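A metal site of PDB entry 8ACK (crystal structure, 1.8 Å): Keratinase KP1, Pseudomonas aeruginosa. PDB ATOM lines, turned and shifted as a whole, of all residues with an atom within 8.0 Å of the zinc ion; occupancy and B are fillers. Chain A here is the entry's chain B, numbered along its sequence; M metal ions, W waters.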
ATOM      1  N   ILE A 354     -25.514  19.772 -22.650  1.00  0.00           N
ATOM      2  CA  ILE A 354     -24.216  19.324 -23.117  1.00  0.00           C
ATOM      3  C   ILE A 354     -23.146  20.124 -22.395  1.00  0.00           C
ATOM      4  O   ILE A 354     -23.271  21.353 -22.270  1.00  0.00           O
ATOM      5  CB  ILE A 354     -24.076  19.483 -24.651  1.00  0.00           C
ATOM      6  CG1 ILE A 354     -25.175  18.695 -25.384  1.00  0.00           C
ATOM      7  CG2 ILE A 354     -22.699  19.037 -25.103  1.00  0.00           C
ATOM      8  CD1 ILE A 354     -25.299  19.080 -26.896  1.00  0.00           C
ATOM      9  N   TYR A 355     -22.120  19.453 -21.887  1.00  0.00           N
ATOM     10  CA  TYR A 355     -21.053  20.164 -21.185  1.00  0.00           C
ATOM     11  C   TYR A 355     -20.508  21.272 -22.053  1.00  0.00           C
ATOM     12  O   TYR A 355     -20.156  21.051 -23.221  1.00  0.00           O
ATOM     13  CB  TYR A 355     -19.913  19.221 -20.805  1.00  0.00           C
ATOM     14  CG  TYR A 355     -20.196  18.251 -19.688  1.00  0.00           C
ATOM     15  CD1 TYR A 355     -21.471  18.080 -19.158  1.00  0.00           C
ATOM     16  CD2 TYR A 355     -19.160  17.486 -19.165  1.00  0.00           C
ATOM     17  CE1 TYR A 355     -21.697  17.165 -18.127  1.00  0.00           C
ATOM     18  CE2 TYR A 355     -19.374  16.590 -18.146  1.00  0.00           C
ATOM     19  CZ  TYR A 355     -20.636  16.427 -17.633  1.00  0.00           C
ATOM     20  OH  TYR A 355     -20.806  15.508 -16.627  1.00  0.00           O
ATOM     21  N   ASP A 356     -20.388  22.478 -21.468  1.00  0.00           N
ATOM     22  CA  ASP A 356     -19.984  23.688 -22.204  1.00  0.00           C
ATOM     23  C   ASP A 356     -18.460  23.753 -22.333  1.00  0.00           C
ATOM     24  O   ASP A 356     -17.793  24.681 -21.851  1.00  0.00           O
ATOM     25  CB  ASP A 356     -20.545  24.934 -21.537  1.00  0.00           C
ATOM     26  CG  ASP A 356     -20.145  26.203 -22.258  1.00  0.00           C
ATOM     27  OD1 ASP A 356     -20.097  26.184 -23.512  1.00  0.00           O
ATOM     28  OD2 ASP A 356     -19.865  27.213 -21.588  1.00  0.00           O
ATOM     29  N   GLY A 357     -17.912  22.790 -23.070  1.00  0.00           N
ATOM     30  CA  GLY A 357     -16.476  22.690 -23.248  1.00  0.00           C
ATOM     31  C   GLY A 357     -15.831  23.918 -23.863  1.00  0.00           C
ATOM     32  O   GLY A 357     -14.682  24.240 -23.528  1.00  0.00           O
ATOM     33  N   ASP A 358     -16.523  24.607 -24.769  1.00  0.00           N
ATOM     34  CA  ASP A 358     -15.943  25.783 -25.409  1.00  0.00           C
ATOM     35  C   ASP A 358     -16.100  27.056 -24.576  1.00  0.00           C
ATOM     36  O   ASP A 358     -15.604  28.109 -24.987  1.00  0.00           O
ATOM     37  CB  ASP A 358     -16.521  26.007 -26.825  1.00  0.00           C
ATOM     38  CG  ASP A 358     -18.045  26.210 -26.829  1.00  0.00           C
ATOM     39  OD1 ASP A 358     -18.695  26.149 -25.771  1.00  0.00           O
ATOM     40  OD2 ASP A 358     -18.604  26.397 -27.933  1.00  0.00           O
ATOM     41  N   GLY A 359     -16.739  26.972 -23.415  1.00  0.00           N
ATOM     42  CA  GLY A 359     -16.930  28.150 -22.599  1.00  0.00           C
ATOM     43  C   GLY A 359     -17.852  29.177 -23.212  1.00  0.00           C
ATOM     44  O   GLY A 359     -17.907  30.305 -22.718  1.00  0.00           O
ATOM     45  N   SER A 360     -18.579  28.821 -24.277  1.00  0.00           N
ATOM     46  CA  SER A 360     -19.413  29.802 -24.962  1.00  0.00           C
ATOM     47  C   SER A 360     -20.558  30.299 -24.096  1.00  0.00           C
ATOM     48  O   SER A 360     -21.084  31.387 -24.349  1.00  0.00           O
ATOM     49  CB  SER A 360     -19.965  29.194 -26.258  1.00  0.00           C
ATOM     50  OG  SER A 360     -20.786  28.073 -25.951  1.00  0.00           O
ATOM     51  N   ASP A 361     -20.993  29.523 -23.107  1.00  0.00           N
ATOM     52  CA  ASP A 361     -22.084  29.941 -22.246  1.00  0.00           C
ATOM     53  C   ASP A 361     -21.611  30.486 -20.905  1.00  0.00           C
ATOM     54  O   ASP A 361     -22.089  31.528 -20.475  1.00  0.00           O
ATOM     55  CB  ASP A 361     -23.055  28.784 -21.996  1.00  0.00           C
ATOM     56  CG  ASP A 361     -23.716  28.287 -23.271  1.00  0.00           C
ATOM     57  OD1 ASP A 361     -23.904  29.090 -24.208  1.00  0.00           O
ATOM     58  OD2 ASP A 361     -24.064  27.093 -23.324  1.00  0.00           O
ATOM     59  N   PHE A 362     -20.641  29.828 -20.267  1.00  0.00           N
ATOM     60  CA  PHE A 362     -20.260  30.153 -18.901  1.00  0.00           C
ATOM     61  C   PHE A 362     -18.799  30.586 -18.758  1.00  0.00           C
ATOM     62  O   PHE A 362     -18.355  30.845 -17.646  1.00  0.00           O
ATOM     63  CB  PHE A 362     -20.541  28.971 -17.972  1.00  0.00           C
ATOM     64  CG  PHE A 362     -21.915  28.397 -18.120  1.00  0.00           C
ATOM     65  CD1 PHE A 362     -23.017  29.023 -17.532  1.00  0.00           C
ATOM     66  CD2 PHE A 362     -22.134  27.246 -18.878  1.00  0.00           C
ATOM     67  CE1 PHE A 362     -24.291  28.504 -17.680  1.00  0.00           C
ATOM     68  CE2 PHE A 362     -23.408  26.727 -19.025  1.00  0.00           C
ATOM     69  CZ  PHE A 362     -24.490  27.354 -18.434  1.00  0.00           C
ATOM     70  N   GLY A 363     -18.049  30.668 -19.865  1.00  0.00           N
ATOM     71  CA  GLY A 363     -16.744  31.286 -19.833  1.00  0.00           C
ATOM     72  C   GLY A 363     -15.614  30.420 -19.307  1.00  0.00           C
ATOM     73  O   GLY A 363     -14.484  30.908 -19.201  1.00  0.00           O
ATOM     74  N   LEU A 364     -15.864  29.157 -18.981  1.00  0.00           N
ATOM     75  CA  LEU A 364     -14.818  28.222 -18.592  1.00  0.00           C
ATOM     76  C   LEU A 364     -14.595  27.238 -19.737  1.00  0.00           C
ATOM     77  O   LEU A 364     -15.520  26.515 -20.127  1.00  0.00           O
ATOM     78  CB  LEU A 364     -15.180  27.490 -17.312  1.00  0.00           C
ATOM     79  CG  LEU A 364     -14.142  26.497 -16.773  1.00  0.00           C
ATOM     80  CD1 LEU A 364     -12.781  27.143 -16.616  1.00  0.00           C
ATOM     81  CD2 LEU A 364     -14.609  25.895 -15.440  1.00  0.00           C
ATOM     82  N   SER A 370     -11.879  19.703 -25.922  1.00  0.00           N
ATOM     83  CA  SER A 370     -13.191  19.687 -25.282  1.00  0.00           C
ATOM     84  C   SER A 370     -14.238  20.394 -26.147  1.00  0.00           C
ATOM     85  O   SER A 370     -15.412  20.021 -26.151  1.00  0.00           O
ATOM     86  CB  SER A 370     -13.095  20.327 -23.902  1.00  0.00           C
ATOM     87  OG  SER A 370     -12.060  19.710 -23.142  1.00  0.00           O
ATOM     88  N   ALA A 371     -13.837  21.458 -26.851  1.00  0.00           N
ATOM     89  CA  ALA A 371     -14.760  22.102 -27.766  1.00  0.00           C
ATOM     90  C   ALA A 371     -15.214  21.123 -28.847  1.00  0.00           C
ATOM     91  O   ALA A 371     -16.395  21.073 -29.206  1.00  0.00           O
ATOM     92  CB  ALA A 371     -14.124  23.343 -28.388  1.00  0.00           C
ATOM     93  N   GLU A 374     -17.804  18.696 -27.392  1.00  0.00           N
ATOM     94  CA  GLU A 374     -19.071  19.387 -27.264  1.00  0.00           C
ATOM     95  C   GLU A 374     -19.740  19.567 -28.628  1.00  0.00           C
ATOM     96  O   GLU A 374     -20.951  19.327 -28.768  1.00  0.00           O
ATOM     97  CB  GLU A 374     -18.858  20.745 -26.601  1.00  0.00           C
ATOM     98  CG  GLU A 374     -20.085  21.627 -26.645  1.00  0.00           C
ATOM     99  CD  GLU A 374     -19.839  23.021 -26.104  1.00  0.00           C
ATOM    100  OE1 GLU A 374     -18.740  23.577 -26.308  1.00  0.00           O
ATOM    101  OE2 GLU A 374     -20.740  23.546 -25.437  1.00  0.00           O
ATOM    102  N   ARG A 375     -18.954  19.932 -29.641  1.00  0.00           N
ATOM    103  CA  ARG A 375     -19.482  20.123 -30.996  1.00  0.00           C
ATOM    104  C   ARG A 375     -20.036  18.829 -31.593  1.00  0.00           C
ATOM    105  O   ARG A 375     -21.017  18.857 -32.348  1.00  0.00           O
ATOM    106  CB  ARG A 375     -18.379  20.699 -31.884  1.00  0.00           C
ATOM    107  CG  ARG A 375     -18.831  21.419 -33.123  1.00  0.00           C
ATOM    108  CD  ARG A 375     -17.627  22.095 -33.766  1.00  0.00           C
ATOM    109  NE  ARG A 375     -17.102  23.143 -32.897  1.00  0.00           N
ATOM    110  CZ  ARG A 375     -15.889  23.140 -32.333  1.00  0.00           C
ATOM    111  NH1 ARG A 375     -15.054  22.124 -32.560  1.00  0.00           N
ATOM    112  NH2 ARG A 375     -15.516  24.150 -31.567  1.00  0.00           N
ATOM    113  N   GLU A 378     -23.373  18.384 -29.958  1.00  0.00           N
ATOM    114  CA  GLU A 378     -24.293  19.401 -30.475  1.00  0.00           C
ATOM    115  C   GLU A 378     -24.826  19.015 -31.843  1.00  0.00           C
ATOM    116  O   GLU A 378     -26.018  19.146 -32.119  1.00  0.00           O
ATOM    117  CB  GLU A 378     -23.604  20.774 -30.566  1.00  0.00           C
ATOM    118  CG  GLU A 378     -23.350  21.469 -29.219  1.00  0.00           C
ATOM    119  CD  GLU A 378     -22.493  22.722 -29.367  1.00  0.00           C
ATOM    120  OE1 GLU A 378     -22.390  23.511 -28.397  1.00  0.00           O
ATOM    121  OE2 GLU A 378     -21.921  22.932 -30.460  1.00  0.00           O
ATOM    122  N   GLU A 389     -28.636  22.600 -25.023  1.00  0.00           N
ATOM    123  CA  GLU A 389     -27.981  23.814 -24.567  1.00  0.00           C
ATOM    124  C   GLU A 389     -26.877  23.448 -23.565  1.00  0.00           C
ATOM    125  O   GLU A 389     -26.754  22.298 -23.127  1.00  0.00           O
ATOM    126  CB  GLU A 389     -28.986  24.787 -23.944  1.00  0.00           C
ATOM    127  CG  GLU A 389     -29.626  24.269 -22.673  1.00  0.00           C
ATOM    128  CD  GLU A 389     -30.795  25.121 -22.239  1.00  0.00           C
ATOM    129  OE1 GLU A 389     -31.924  24.896 -22.737  1.00  0.00           O
ATOM    130  OE2 GLU A 389     -30.588  26.033 -21.393  1.00  0.00           O
ATOM    131  N   GLY A 390     -26.084  24.450 -23.216  1.00  0.00           N
ATOM    132  CA  GLY A 390     -24.899  24.177 -22.425  1.00  0.00           C
ATOM    133  C   GLY A 390     -25.185  24.053 -20.936  1.00  0.00           C
ATOM    134  O   GLY A 390     -26.198  24.521 -20.416  1.00  0.00           O
ATOM    135  N   THR A 391     -24.267  23.387 -20.244  1.00  0.00           N
ATOM    136  CA  THR A 391     -24.281  23.333 -18.794  1.00  0.00           C
ATOM    137  C   THR A 391     -22.846  23.514 -18.292  1.00  0.00           C
ATOM    138  O   THR A 391     -21.887  23.279 -19.026  1.00  0.00           O
ATOM    139  CB  THR A 391     -24.916  22.040 -18.275  1.00  0.00           C
ATOM    140  OG1 THR A 391     -25.040  22.104 -16.846  1.00  0.00           O
ATOM    141  CG2 THR A 391     -24.086  20.817 -18.655  1.00  0.00           C
HETATM  142 ZN    ZN M   1     -20.614  25.798 -25.470  1.00  0.00          ZN
HETATM  143  O   HOH W   1     -22.537  25.703 -25.027  1.00  0.00           O
HETATM  144  O   HOH W   2     -21.071  25.861 -27.777  1.00  0.00           O
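Within 4 Å of the zinc ion: Asp 356, Asp 358, Ser 360 and Glu 374.
Water W2 bridges OD2 of Asp 358 (2.5 Å) and OE1 of Glu 378 (2.8 Å).
OD1 of Asp 358 binds the zinc ion (2.0 Å). Water W1 is bound to the zinc ion (2.0 Å). OD1 of Asp 356 is bound to the zinc ion (2.1 Å). The zinc ion is bound by the side-chain carboxylate (OE2) of Glu 374, 2.3 Å away. OG of Ser 360 is bound to the zinc ion. Water W2 binds the zinc ion (2.4 Å).
The side-chain carboxylate (OD2) of Asp 356 is in hydrogen-bond range of the backbone NH (N) of Phe 362 (3.0 Å). The backbone NH of Gly 357 is in hydrogen-bond range of the side-chain carboxylate of Glu 374 (3.4 Å). The backbone NH (N) of Asp 356 is in hydrogen-bond range of the backbone carbonyl oxygen (O) of Thr 391, 3.0 Å away. The side-chain carboxylate (OD2) of Asp 356 lies within hydrogen-bond range of the backbone NH (N) of Asp 361 (3.0 Å). OD1 of Asp 356 lies close to N of Gly 359 (3.5 Å).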
